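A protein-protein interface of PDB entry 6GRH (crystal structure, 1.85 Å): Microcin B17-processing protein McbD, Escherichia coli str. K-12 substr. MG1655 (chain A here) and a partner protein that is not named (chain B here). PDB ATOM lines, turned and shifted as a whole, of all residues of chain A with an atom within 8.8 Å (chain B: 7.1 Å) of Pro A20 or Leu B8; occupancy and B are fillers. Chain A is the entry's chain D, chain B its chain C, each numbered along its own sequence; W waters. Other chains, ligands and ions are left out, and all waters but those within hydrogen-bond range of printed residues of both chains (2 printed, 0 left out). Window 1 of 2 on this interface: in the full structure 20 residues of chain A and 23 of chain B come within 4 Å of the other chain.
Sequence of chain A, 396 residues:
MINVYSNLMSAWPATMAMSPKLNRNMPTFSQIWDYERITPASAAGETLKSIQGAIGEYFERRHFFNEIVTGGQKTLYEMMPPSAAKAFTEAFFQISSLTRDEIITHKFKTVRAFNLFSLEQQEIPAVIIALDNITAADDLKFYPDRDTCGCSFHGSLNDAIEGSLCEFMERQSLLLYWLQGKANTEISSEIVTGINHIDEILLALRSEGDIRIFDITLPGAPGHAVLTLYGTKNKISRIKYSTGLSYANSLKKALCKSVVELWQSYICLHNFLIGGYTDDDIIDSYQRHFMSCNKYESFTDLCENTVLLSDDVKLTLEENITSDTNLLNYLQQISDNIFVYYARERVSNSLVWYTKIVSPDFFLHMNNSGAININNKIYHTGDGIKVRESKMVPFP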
ATOM      1  N   MET A   1     -25.058  32.322  -2.451  1.00  0.00           N
ATOM      2  CA  MET A   1     -23.952  32.594  -1.485  1.00  0.00           C
ATOM      3  C   MET A   1     -22.608  32.324  -2.137  1.00  0.00           C
ATOM      4  O   MET A   1     -22.546  31.703  -3.189  1.00  0.00           O
ATOM      5  CB  MET A   1     -24.117  31.771  -0.200  1.00  0.00           C
ATOM      6  CG  MET A   1     -25.078  32.450   0.760  1.00  0.00           C
ATOM      7  SD  MET A   1     -25.567  31.414   2.135  1.00  0.00           S
ATOM      8  CE  MET A   1     -26.693  30.238   1.380  1.00  0.00           C
ATOM      9  N   ILE A   2     -21.541  32.775  -1.473  1.00  0.00           N
ATOM     10  CA  ILE A   2     -20.204  32.920  -2.052  1.00  0.00           C
ATOM     11  C   ILE A   2     -20.281  33.944  -3.172  1.00  0.00           C
ATOM     12  O   ILE A   2     -20.012  35.127  -2.940  1.00  0.00           O
ATOM     13  CB  ILE A   2     -19.580  31.593  -2.496  1.00  0.00           C
ATOM     14  CG1 ILE A   2     -19.298  30.749  -1.265  1.00  0.00           C
ATOM     15  CG2 ILE A   2     -18.291  31.830  -3.283  1.00  0.00           C
ATOM     16  CD1 ILE A   2     -18.926  29.323  -1.580  1.00  0.00           C
ATOM     17  N   ASN A   3     -20.734  33.513  -4.341  1.00  0.00           N
ATOM     18  CA  ASN A   3     -20.906  34.384  -5.503  1.00  0.00           C
ATOM     19  C   ASN A   3     -19.653  35.156  -5.887  1.00  0.00           C
ATOM     20  O   ASN A   3     -19.623  36.376  -5.829  1.00  0.00           O
ATOM     21  CB  ASN A   3     -22.091  35.307  -5.272  1.00  0.00           C
ATOM     22  CG  ASN A   3     -23.358  34.548  -4.973  1.00  0.00           C
ATOM     23  OD1 ASN A   3     -23.839  34.504  -3.809  1.00  0.00           O
ATOM     24  ND2 ASN A   3     -23.896  33.889  -6.007  1.00  0.00           N
ATOM     25  N   ALA A  17     -20.708  29.607  -6.994  1.00  0.00           N
ATOM     26  CA  ALA A  17     -21.879  29.864  -6.162  1.00  0.00           C
ATOM     27  C   ALA A  17     -22.235  28.648  -5.290  1.00  0.00           C
ATOM     28  O   ALA A  17     -22.147  27.506  -5.716  1.00  0.00           O
ATOM     29  CB  ALA A  17     -23.051  30.266  -7.031  1.00  0.00           C
ATOM     30  N   MET A  18     -22.581  28.930  -4.044  1.00  0.00           N
ATOM     31  CA  MET A  18     -23.201  27.958  -3.163  1.00  0.00           C
ATOM     32  C   MET A  18     -24.686  28.275  -3.203  1.00  0.00           C
ATOM     33  O   MET A  18     -25.097  29.402  -2.940  1.00  0.00           O
ATOM     34  CB  MET A  18     -22.639  28.116  -1.765  1.00  0.00           C
ATOM     35  CG  MET A  18     -23.198  27.145  -0.753  1.00  0.00           C
ATOM     36  SD  MET A  18     -22.446  27.491   0.852  1.00  0.00           S
ATOM     37  CE  MET A  18     -23.745  28.373   1.691  1.00  0.00           C
ATOM     38  N   SER A  19     -25.489  27.297  -3.559  1.00  0.00           N
ATOM     39  CA  SER A  19     -26.930  27.499  -3.641  1.00  0.00           C
ATOM     40  C   SER A  19     -27.629  27.681  -2.266  1.00  0.00           C
ATOM     41  O   SER A  19     -27.386  26.921  -1.342  1.00  0.00           O
ATOM     42  CB  SER A  19     -27.580  26.339  -4.394  1.00  0.00           C
ATOM     43  OG  SER A  19     -28.984  26.542  -4.405  1.00  0.00           O
ATOM     44  N   PRO A  20     -28.501  28.699  -2.141  1.00  0.00           N
ATOM     45  CA  PRO A  20     -29.414  28.745  -1.011  1.00  0.00           C
ATOM     46  C   PRO A  20     -30.291  27.511  -0.962  1.00  0.00           C
ATOM     47  O   PRO A  20     -30.543  26.882  -2.013  1.00  0.00           O
ATOM     48  CB  PRO A  20     -30.321  29.945  -1.332  1.00  0.00           C
ATOM     49  CG  PRO A  20     -29.547  30.766  -2.267  1.00  0.00           C
ATOM     50  CD  PRO A  20     -28.738  29.816  -3.080  1.00  0.00           C
ATOM     51  N   LYS A  21     -30.754  27.169   0.239  1.00  0.00           N
ATOM     52  CA  LYS A  21     -31.707  26.098   0.440  1.00  0.00           C
ATOM     53  C   LYS A  21     -32.562  26.451   1.652  1.00  0.00           C
ATOM     54  O   LYS A  21     -32.069  27.041   2.616  1.00  0.00           O
ATOM     55  CB  LYS A  21     -30.972  24.776   0.673  1.00  0.00           C
ATOM     56  CG  LYS A  21     -30.323  24.688   2.051  1.00  0.00           C
ATOM     57  CD  LYS A  21     -29.393  23.487   2.167  1.00  0.00           C
ATOM     58  CE  LYS A  21     -28.485  23.626   3.375  1.00  0.00           C
ATOM     59  NZ  LYS A  21     -27.404  22.611   3.474  1.00  0.00           N
ATOM     60  N   LEU A  22     -33.845  26.109   1.601  1.00  0.00           N
ATOM     61  CA  LEU A  22     -34.740  26.361   2.720  1.00  0.00           C
ATOM     62  C   LEU A  22     -34.499  25.414   3.901  1.00  0.00           C
ATOM     63  O   LEU A  22     -34.591  25.843   5.046  1.00  0.00           O
ATOM     64  CB  LEU A  22     -36.196  26.255   2.287  1.00  0.00           C
ATOM     65  CG  LEU A  22     -36.738  27.243   1.257  1.00  0.00           C
ATOM     66  CD1 LEU A  22     -38.236  27.067   1.097  1.00  0.00           C
ATOM     67  CD2 LEU A  22     -36.439  28.676   1.661  1.00  0.00           C
ATOM     68  N   ASN A  23     -34.189  24.155   3.595  1.00  0.00           N
ATOM     69  CA  ASN A  23     -34.113  23.046   4.557  1.00  0.00           C
ATOM     70  C   ASN A  23     -32.679  22.866   5.092  1.00  0.00           C
ATOM     71  O   ASN A  23     -31.753  22.503   4.339  1.00  0.00           O
ATOM     72  CB  ASN A  23     -34.563  21.767   3.835  1.00  0.00           C
ATOM     73  CG  ASN A  23     -34.666  20.575   4.746  1.00  0.00           C
ATOM     74  OD1 ASN A  23     -34.205  20.597   5.888  1.00  0.00           O
ATOM     75  ND2 ASN A  23     -35.286  19.515   4.244  1.00  0.00           N
ATOM     76  N   MET A  26     -31.022  19.485   4.293  1.00  0.00           N
ATOM     77  CA  MET A  26     -30.617  19.011   2.980  1.00  0.00           C
ATOM     78  C   MET A  26     -29.137  19.330   2.802  1.00  0.00           C
ATOM     79  O   MET A  26     -28.620  20.245   3.452  1.00  0.00           O
ATOM     80  CB  MET A  26     -31.474  19.591   1.864  1.00  0.00           C
ATOM     81  CG  MET A  26     -32.843  18.892   1.717  1.00  0.00           C
ATOM     82  SD  MET A  26     -32.742  17.187   1.106  1.00  0.00           S
ATOM     83  CE  MET A  26     -34.459  16.728   0.798  1.00  0.00           C
ATOM     84  N   PRO A  27     -28.439  18.563   1.948  1.00  0.00           N
ATOM     85  CA  PRO A  27     -27.029  18.867   1.678  1.00  0.00           C
ATOM     86  C   PRO A  27     -26.885  20.211   0.974  1.00  0.00           C
ATOM     87  O   PRO A  27     -27.803  20.671   0.337  1.00  0.00           O
ATOM     88  CB  PRO A  27     -26.552  17.723   0.783  1.00  0.00           C
ATOM     89  CG  PRO A  27     -27.736  16.918   0.425  1.00  0.00           C
ATOM     90  CD  PRO A  27     -28.905  17.345   1.263  1.00  0.00           C
ATOM     91  N   THR A  28     -25.738  20.834   1.161  1.00  0.00           N
ATOM     92  CA  THR A  28     -25.379  22.034   0.465  1.00  0.00           C
ATOM     93  C   THR A  28     -24.866  21.615  -0.900  1.00  0.00           C
ATOM     94  O   THR A  28     -24.156  20.615  -1.009  1.00  0.00           O
ATOM     95  CB  THR A  28     -24.277  22.781   1.239  1.00  0.00           C
ATOM     96  OG1 THR A  28     -24.818  23.263   2.470  1.00  0.00           O
ATOM     97  CG2 THR A  28     -23.706  23.977   0.457  1.00  0.00           C
ATOM     98  N   PHE A  29     -25.185  22.428  -1.911  1.00  0.00           N
ATOM     99  CA  PHE A  29     -24.776  22.228  -3.274  1.00  0.00           C
ATOM    100  C   PHE A  29     -23.981  23.450  -3.695  1.00  0.00           C
ATOM    101  O   PHE A  29     -24.452  24.587  -3.519  1.00  0.00           O
ATOM    102  CB  PHE A  29     -26.020  22.098  -4.134  1.00  0.00           C
ATOM    103  CG  PHE A  29     -25.736  21.927  -5.604  1.00  0.00           C
ATOM    104  CD1 PHE A  29     -25.428  20.664  -6.142  1.00  0.00           C
ATOM    105  CD2 PHE A  29     -25.791  23.022  -6.470  1.00  0.00           C
ATOM    106  CE1 PHE A  29     -25.170  20.516  -7.504  1.00  0.00           C
ATOM    107  CE2 PHE A  29     -25.557  22.872  -7.834  1.00  0.00           C
ATOM    108  CZ  PHE A  29     -25.249  21.620  -8.352  1.00  0.00           C
ATOM    109  N   SER A  30     -22.787  23.227  -4.229  1.00  0.00           N
ATOM    110  CA  SER A  30     -21.920  24.313  -4.709  1.00  0.00           C
ATOM    111  C   SER A  30     -21.528  24.015  -6.136  1.00  0.00           C
ATOM    112  O   SER A  30     -21.296  22.870  -6.481  1.00  0.00           O
ATOM    113  CB  SER A  30     -20.660  24.459  -3.850  1.00  0.00           C
ATOM    114  OG  SER A  30     -20.981  24.840  -2.518  1.00  0.00           O
ATOM    115  N   TRP A 263     -28.369  12.043  -4.943  1.00  0.00           N
ATOM    116  CA  TRP A 263     -29.082  13.308  -4.818  1.00  0.00           C
ATOM    117  C   TRP A 263     -28.516  14.391  -5.751  1.00  0.00           C
ATOM    118  O   TRP A 263     -29.261  15.108  -6.423  1.00  0.00           O
ATOM    119  CB  TRP A 263     -29.036  13.799  -3.377  1.00  0.00           C
ATOM    120  CG  TRP A 263     -29.767  15.074  -3.217  1.00  0.00           C
ATOM    121  CD1 TRP A 263     -31.102  15.238  -3.111  1.00  0.00           C
ATOM    122  CD2 TRP A 263     -29.191  16.370  -3.202  1.00  0.00           C
ATOM    123  NE1 TRP A 263     -31.403  16.581  -3.018  1.00  0.00           N
ATOM    124  CE2 TRP A 263     -30.243  17.294  -3.067  1.00  0.00           C
ATOM    125  CE3 TRP A 263     -27.879  16.840  -3.296  1.00  0.00           C
ATOM    126  CZ2 TRP A 263     -30.034  18.674  -2.999  1.00  0.00           C
ATOM    127  CZ3 TRP A 263     -27.656  18.222  -3.237  1.00  0.00           C
ATOM    128  CH2 TRP A 263     -28.734  19.124  -3.087  1.00  0.00           C
ATOM    129  N   ILE A 267     -30.785  16.018  -8.588  1.00  0.00           N
ATOM    130  CA  ILE A 267     -31.160  17.423  -8.577  1.00  0.00           C
ATOM    131  C   ILE A 267     -30.601  18.215  -9.770  1.00  0.00           C
ATOM    132  O   ILE A 267     -31.299  19.092 -10.287  1.00  0.00           O
ATOM    133  CB  ILE A 267     -30.853  18.098  -7.213  1.00  0.00           C
ATOM    134  CG1 ILE A 267     -31.758  19.308  -7.023  1.00  0.00           C
ATOM    135  CG2 ILE A 267     -29.388  18.471  -7.077  1.00  0.00           C
ATOM    136  CD1 ILE A 267     -33.218  18.950  -6.897  1.00  0.00           C
ATOM    137  N   ASN A 271     -33.129  20.059 -12.274  1.00  0.00           N
ATOM    138  CA  ASN A 271     -33.041  21.495 -12.494  1.00  0.00           C
ATOM    139  C   ASN A 271     -32.820  21.871 -13.956  1.00  0.00           C
ATOM    140  O   ASN A 271     -33.334  22.902 -14.418  1.00  0.00           O
ATOM    141  CB  ASN A 271     -31.937  22.107 -11.640  1.00  0.00           C
ATOM    142  CG  ASN A 271     -32.345  22.253 -10.184  1.00  0.00           C
ATOM    143  OD1 ASN A 271     -33.533  22.242  -9.850  1.00  0.00           O
ATOM    144  ND2 ASN A 271     -31.368  22.408  -9.323  1.00  0.00           N
ATOM    145  N   ILE A 274     -36.522  21.370 -15.391  1.00  0.00           N
ATOM    146  CA  ILE A 274     -37.497  22.430 -15.049  1.00  0.00           C
ATOM    147  C   ILE A 274     -37.015  23.808 -15.519  1.00  0.00           C
ATOM    148  O   ILE A 274     -37.805  24.745 -15.627  1.00  0.00           O
ATOM    149  CB  ILE A 274     -37.858  22.462 -13.543  1.00  0.00           C
ATOM    150  CG1 ILE A 274     -36.659  22.851 -12.667  1.00  0.00           C
ATOM    151  CG2 ILE A 274     -38.418  21.115 -13.119  1.00  0.00           C
ATOM    152  CD1 ILE A 274     -37.049  23.305 -11.281  1.00  0.00           C
ATOM    153  N   LEU B   6     -39.279  26.876  -9.025  1.00  0.00           N
ATOM    154  CA  LEU B   6     -38.095  27.644  -9.337  1.00  0.00           C
ATOM    155  C   LEU B   6     -36.997  27.128  -8.415  1.00  0.00           C
ATOM    156  O   LEU B   6     -37.191  27.051  -7.190  1.00  0.00           O
ATOM    157  CB  LEU B   6     -38.332  29.126  -9.041  1.00  0.00           C
ATOM    158  CG  LEU B   6     -37.086  30.027  -8.998  1.00  0.00           C
ATOM    159  CD1 LEU B   6     -36.400  30.010 -10.358  1.00  0.00           C
ATOM    160  CD2 LEU B   6     -37.481  31.427  -8.577  1.00  0.00           C
ATOM    161  N   SER B   7     -35.848  26.817  -8.994  1.00  0.00           N
ATOM    162  CA  SER B   7     -34.689  26.424  -8.217  1.00  0.00           C
ATOM    163  C   SER B   7     -33.945  27.671  -7.744  1.00  0.00           C
ATOM    164  O   SER B   7     -33.657  28.557  -8.543  1.00  0.00           O
ATOM    165  CB  SER B   7     -33.739  25.571  -9.056  1.00  0.00           C
ATOM    166  OG  SER B   7     -32.578  25.283  -8.282  1.00  0.00           O
ATOM    167  N   LEU B   8     -33.576  27.708  -6.467  1.00  0.00           N
ATOM    168  CA  LEU B   8     -32.743  28.799  -5.960  1.00  0.00           C
ATOM    169  C   LEU B   8     -31.323  28.899  -6.606  1.00  0.00           C
ATOM    170  O   LEU B   8     -30.685  29.951  -6.525  1.00  0.00           O
ATOM    171  CB  LEU B   8     -32.671  28.730  -4.426  1.00  0.00           C
ATOM    172  CG  LEU B   8     -33.994  29.025  -3.725  1.00  0.00           C
ATOM    173  CD1 LEU B   8     -33.908  28.775  -2.220  1.00  0.00           C
ATOM    174  CD2 LEU B   8     -34.443  30.453  -4.022  1.00  0.00           C
ATOM    175  N   VAL B   9     -30.861  27.810  -7.219  1.00  0.00           N
ATOM    176  CA  VAL B   9     -29.646  27.805  -8.033  1.00  0.00           C
ATOM    177  C   VAL B   9     -29.687  28.889  -9.106  1.00  0.00           C
ATOM    178  O   VAL B   9     -28.694  29.572  -9.342  1.00  0.00           O
ATOM    179  CB  VAL B   9     -29.447  26.439  -8.703  1.00  0.00           C
ATOM    180  CG1 VAL B   9     -28.218  26.460  -9.612  1.00  0.00           C
ATOM    181  CG2 VAL B   9     -29.336  25.343  -7.639  1.00  0.00           C
ATOM    182  N   GLU B  10     -30.857  29.050  -9.722  1.00  0.00           N
ATOM    183  CA  GLU B  10     -31.064  30.029 -10.802  1.00  0.00           C
ATOM    184  C   GLU B  10     -30.992  31.455 -10.252  1.00  0.00           C
ATOM    185  O   GLU B  10     -30.462  32.347 -10.912  1.00  0.00           O
ATOM    186  CB  GLU B  10     -32.411  29.810 -11.517  1.00  0.00           C
ATOM    187  CG  GLU B  10     -32.566  28.460 -12.203  1.00  0.00           C
ATOM    188  CD  GLU B  10     -31.876  28.359 -13.561  1.00  0.00           C
ATOM    189  OE1 GLU B  10     -31.214  29.334 -13.999  1.00  0.00           O
ATOM    190  OE2 GLU B  10     -32.023  27.288 -14.227  1.00  0.00           O
ATOM    191  N   VAL B  11     -31.531  31.638  -9.052  1.00  0.00           N
ATOM    192  CA  VAL B  11     -31.521  32.914  -8.366  1.00  0.00           C
ATOM    193  C   VAL B  11     -30.108  33.331  -7.982  1.00  0.00           C
ATOM    194  O   VAL B  11     -29.705  34.473  -8.256  1.00  0.00           O
ATOM    195  CB  VAL B  11     -32.456  32.896  -7.129  1.00  0.00           C
ATOM    196  CG1 VAL B  11     -32.281  34.138  -6.273  1.00  0.00           C
ATOM    197  CG2 VAL B  11     -33.881  32.753  -7.611  1.00  0.00           C
ATOM    198  N   THR B  12     -29.338  32.418  -7.385  1.00  0.00           N
ATOM    199  CA  THR B  12     -28.045  32.815  -6.826  1.00  0.00           C
ATOM    200  C   THR B  12     -27.027  33.274  -7.902  1.00  0.00           C
ATOM    201  O   THR B  12     -26.113  34.028  -7.612  1.00  0.00           O
ATOM    202  CB  THR B  12     -27.448  31.729  -5.916  1.00  0.00           C
ATOM    203  OG1 THR B  12     -26.478  32.313  -5.037  1.00  0.00           O
ATOM    204  CG2 THR B  12     -26.803  30.621  -6.729  1.00  0.00           C
ATOM    205  N   HIS B  13     -27.212  32.816  -9.136  1.00  0.00           N
ATOM    206  CA  HIS B  13     -26.440  33.302 -10.271  1.00  0.00           C
ATOM    207  C   HIS B  13     -26.372  34.843 -10.358  1.00  0.00           C
ATOM    208  O   HIS B  13     -25.377  35.373 -10.828  1.00  0.00           O
ATOM    209  CB  HIS B  13     -27.014  32.691 -11.561  1.00  0.00           C
ATOM    210  CG  HIS B  13     -26.142  32.858 -12.756  1.00  0.00           C
ATOM    211  ND1 HIS B  13     -24.862  32.344 -12.820  1.00  0.00           N
ATOM    212  CD2 HIS B  13     -26.374  33.457 -13.952  1.00  0.00           C
ATOM    213  CE1 HIS B  13     -24.335  32.646 -13.997  1.00  0.00           C
ATOM    214  NE2 HIS B  13     -25.234  33.317 -14.702  1.00  0.00           N
ATOM    215  N   THR B  15     -26.831  36.958  -7.569  1.00  0.00           N
ATOM    216  CA  THR B  15     -26.672  37.539  -6.243  1.00  0.00           C
ATOM    217  C   THR B  15     -25.394  38.376  -6.145  1.00  0.00           C
ATOM    218  O   THR B  15     -24.325  37.965  -6.598  1.00  0.00           O
ATOM    219  CB  THR B  15     -26.702  36.426  -5.165  1.00  0.00           C
ATOM    220  OG1 THR B  15     -28.040  35.930  -5.096  1.00  0.00           O
ATOM    221  CG2 THR B  15     -26.258  36.927  -3.800  1.00  0.00           C
ATOM    222  N   LEU B  20     -26.021  41.011  -0.126  1.00  0.00           N
ATOM    223  CA  LEU B  20     -26.525  39.965   0.742  1.00  0.00           C
ATOM    224  C   LEU B  20     -26.000  40.082   2.171  1.00  0.00           C
ATOM    225  O   LEU B  20     -26.785  39.998   3.114  1.00  0.00           O
ATOM    226  CB  LEU B  20     -26.212  38.606   0.172  1.00  0.00           C
ATOM    227  CG  LEU B  20     -26.700  37.407   0.961  1.00  0.00           C
ATOM    228  CD1 LEU B  20     -28.217  37.441   1.044  1.00  0.00           C
ATOM    229  CD2 LEU B  20     -26.228  36.146   0.254  1.00  0.00           C
ATOM    230  N   ILE B 194     -36.949  34.778   1.884  1.00  0.00           N
ATOM    231  CA  ILE B 194     -35.787  34.147   1.265  1.00  0.00           C
ATOM    232  C   ILE B 194     -34.879  35.282   0.803  1.00  0.00           C
ATOM    233  O   ILE B 194     -35.205  35.968  -0.165  1.00  0.00           O
ATOM    234  CB  ILE B 194     -36.195  33.251   0.080  1.00  0.00           C
ATOM    235  CG1 ILE B 194     -37.144  32.167   0.573  1.00  0.00           C
ATOM    236  CG2 ILE B 194     -34.942  32.647  -0.578  1.00  0.00           C
ATOM    237  CD1 ILE B 194     -37.633  31.273  -0.532  1.00  0.00           C
ATOM    238  N   PHE B 195     -33.746  35.467   1.456  1.00  0.00           N
ATOM    239  CA  PHE B 195     -32.942  36.692   1.235  1.00  0.00           C
ATOM    240  C   PHE B 195     -32.570  36.893  -0.214  1.00  0.00           C
ATOM    241  O   PHE B 195     -32.774  37.971  -0.775  1.00  0.00           O
ATOM    242  CB  PHE B 195     -31.682  36.720   2.081  1.00  0.00           C
ATOM    243  CG  PHE B 195     -31.951  36.861   3.557  1.00  0.00           C
ATOM    244  CD1 PHE B 195     -32.382  38.063   4.084  1.00  0.00           C
ATOM    245  CD2 PHE B 195     -31.782  35.778   4.411  1.00  0.00           C
ATOM    246  CE1 PHE B 195     -32.615  38.200   5.449  1.00  0.00           C
ATOM    247  CE2 PHE B 195     -32.016  35.908   5.781  1.00  0.00           C
ATOM    248  CZ  PHE B 195     -32.438  37.127   6.292  1.00  0.00           C
ATOM    249  N   GLU B 196     -32.041  35.845  -0.827  1.00  0.00           N
ATOM    250  CA  GLU B 196     -31.540  35.990  -2.189  1.00  0.00           C
ATOM    251  C   GLU B 196     -32.644  36.225  -3.207  1.00  0.00           C
ATOM    252  O   GLU B 196     -32.415  36.945  -4.165  1.00  0.00           O
ATOM    253  CB  GLU B 196     -30.633  34.814  -2.562  1.00  0.00           C
ATOM    254  CG  GLU B 196     -29.300  34.913  -1.813  1.00  0.00           C
ATOM    255  CD  GLU B 196     -28.227  33.957  -2.306  1.00  0.00           C
ATOM    256  OE1 GLU B 196     -27.970  33.908  -3.537  1.00  0.00           O
ATOM    257  OE2 GLU B 196     -27.596  33.303  -1.449  1.00  0.00           O
ATOM    258  N   LYS B 197     -33.836  35.669  -2.991  1.00  0.00           N
ATOM    259  CA  LYS B 197     -34.979  35.943  -3.852  1.00  0.00           C
ATOM    260  C   LYS B 197     -35.456  37.391  -3.694  1.00  0.00           C
ATOM    261  O   LYS B 197     -35.894  37.993  -4.671  1.00  0.00           O
ATOM    262  CB  LYS B 197     -36.123  34.989  -3.578  1.00  0.00           C
ATOM    263  CG  LYS B 197     -37.197  35.061  -4.653  1.00  0.00           C
ATOM    264  CD  LYS B 197     -37.611  33.683  -5.083  1.00  0.00           C
ATOM    265  CE  LYS B 197     -38.820  33.732  -5.991  1.00  0.00           C
ATOM    266  NZ  LYS B 197     -40.080  33.296  -5.316  1.00  0.00           N
ATOM    267  N   ASP B 250     -33.001  26.881   7.177  1.00  0.00           N
ATOM    268  CA  ASP B 250     -31.594  27.274   7.096  1.00  0.00           C
ATOM    269  C   ASP B 250     -31.492  28.804   7.108  1.00  0.00           C
ATOM    270  O   ASP B 250     -31.802  29.480   6.102  1.00  0.00           O
ATOM    271  CB  ASP B 250     -30.960  26.705   5.842  1.00  0.00           C
ATOM    272  CG  ASP B 250     -29.407  26.832   5.830  1.00  0.00           C
ATOM    273  OD1 ASP B 250     -28.800  27.774   6.411  1.00  0.00           O
ATOM    274  OD2 ASP B 250     -28.775  25.953   5.189  1.00  0.00           O
ATOM    275  N   ARG B 252     -29.092  30.834   6.905  1.00  0.00           N
ATOM    276  CA  ARG B 252     -28.298  31.464   5.829  1.00  0.00           C
ATOM    277  C   ARG B 252     -29.132  31.856   4.608  1.00  0.00           C
ATOM    278  O   ARG B 252     -28.741  32.760   3.858  1.00  0.00           O
ATOM    279  CB  ARG B 252     -27.156  30.558   5.384  1.00  0.00           C
ATOM    280  CG  ARG B 252     -26.111  30.309   6.460  1.00  0.00           C
ATOM    281  CD  ARG B 252     -25.184  29.146   6.111  1.00  0.00           C
ATOM    282  NE  ARG B 252     -25.904  27.881   5.970  1.00  0.00           N
ATOM    283  CZ  ARG B 252     -25.336  26.704   5.715  1.00  0.00           C
ATOM    284  NH1 ARG B 252     -24.022  26.585   5.576  1.00  0.00           N
ATOM    285  NH2 ARG B 252     -26.093  25.616   5.610  1.00  0.00           N
ATOM    286  N   THR B 253     -30.271  31.202   4.413  1.00  0.00           N
ATOM    287  CA  THR B 253     -31.112  31.425   3.244  1.00  0.00           C
ATOM    288  C   THR B 253     -32.404  32.131   3.567  1.00  0.00           C
ATOM    289  O   THR B 253     -32.859  32.963   2.768  1.00  0.00           O
ATOM    290  CB  THR B 253     -31.415  30.060   2.600  1.00  0.00           C
ATOM    291  OG1 THR B 253     -30.204  29.541   2.066  1.00  0.00           O
ATOM    292  CG2 THR B 253     -32.428  30.138   1.480  1.00  0.00           C
ATOM    293  N   VAL B 254     -33.016  31.768   4.706  1.00  0.00           N
ATOM    294  CA  VAL B 254     -34.401  32.127   5.014  1.00  0.00           C
ATOM    295  C   VAL B 254     -34.566  32.485   6.506  1.00  0.00           C
ATOM    296  O   VAL B 254     -33.914  31.891   7.381  1.00  0.00           O
ATOM    297  CB  VAL B 254     -35.390  31.033   4.518  1.00  0.00           C
ATOM    298  CG1 VAL B 254     -35.084  29.660   5.094  1.00  0.00           C
ATOM    299  CG2 VAL B 254     -36.839  31.388   4.793  1.00  0.00           C
HETATM  300  O   HOH W   1     -33.169  23.182  -6.550  1.00  0.00           O
HETATM  301  O   HOH W   2     -33.677  25.345 -13.121  1.00  0.00           O
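Water W2 bridges OE2 of Glu B10 and O of Asn A271.
Water W1 bridges OG of Ser B7 and ND2 of Asn A271.
CG of Met A1 touches CD2 of Leu B20, 3.9 Å away.
Met A1 touches Arg B252 (SD to CB, 3.7 Å).
Thr B253 touches Met A1 (OG1 to CE, 3.6 Å).
Thr B12 touches Ala A17.
OG1 of Thr B12 touches O of Met A18, 3.8 Å away.
OG of Ser A19 touches CG2 of Val B9, 3.5 Å away.
Pro A20 touches Leu B8 (O to CB, 3.7 Å).
Pro A20 touches Thr B12 (CD to CB, 3.7 Å).
Lys A21 touches Arg B252.
Val B9 touches Asn A271.
The backbone NH of Met A1 lies within hydrogen-bond range of the side-chain hydroxyl of Thr B12 (3.0 Å).
The side-chain carboxylate (OE2) of Glu B196 is in hydrogen-bond range of the backbone NH (N) of Met A1 (2.9 Å).
The backbone carbonyl oxygen (O) of Leu A22 lies within hydrogen-bond range of the backbone NH (N) of Asp B250, 2.9 Å away.
OG1 of Thr B253 is in hydrogen-bond range of N of Lys A21, at 3.0 Å.
The side-chain hydroxyl of Ser B7 sits at hydrogen-bond distance from the side-chain amide nitrogen of Asn A271 (3.3 Å).
O of Thr B12 lies within hydrogen-bond range of ND2 of Asn A3 (2.7 Å).
NZ of Lys A21 is in salt-bridge range of OD2 of Asp B250 (3.999 Å).
The side-chain carboxylate (OE1) of Glu B196 sits at hydrogen-bond distance from the side-chain hydroxyl (OG1) of Thr B12, at 2.6 Å.
The backbone carbonyl oxygen (O) of Met A1 sits at hydrogen-bond distance from the backbone NH (N) of Met A18.
The backbone carbonyl oxygen (O) of Ile A267 lies close to the side-chain amide nitrogen (ND2) of Asn A271, 3.5 Å away.
The backbone carbonyl oxygen (O) of Phe A29 is in hydrogen-bond range of the backbone NH (N) of Ser A19 (2.9 Å).
OG1 of Thr A28 lies within hydrogen-bond range of NZ of Lys A21 (2.8 Å).
The side-chain hydroxyl (OG) of Ser B7 lies close to the backbone NH (N) of Val B9.
Of the 18 printed residues of chain B, 12 touch a printed residue of chain A.
Printed residues of chain B that touch a printed residue of chain A: Ser B7, Leu B8, Val B9, Thr B12, Thr B15, Leu B20, Ile B194, Glu B196, Asp B250, Arg B252, Thr B253 and Val B254.
Of the 19 printed residues of chain A, 9 touch a printed residue of chain B.
Hydrophobic or aromatic side chains of chain A that line the printed part of chain B: Met A1, Ala A17, Pro A20 and Leu A22.
Pro A20 touches four residues of chain B.
Of the printed residues of chain A, Leu B8 touches Ser A19 and Pro A20.
Of chain A, only Asn A271 comes within 4 Å of Ser B7.
Of the printed residues of chain A, Leu B20 touches Met A1.
Of the printed residues of chain A, Glu B196 touches Met A1 and Pro A20.
Of the printed residues of chain A, Arg B252 touches Met A1 (3.7 Å) and Lys A21 (3.8 Å).
Pro A27 touches none of the printed residues of chain B.
Asn A23 touches none of the printed residues of chain B.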
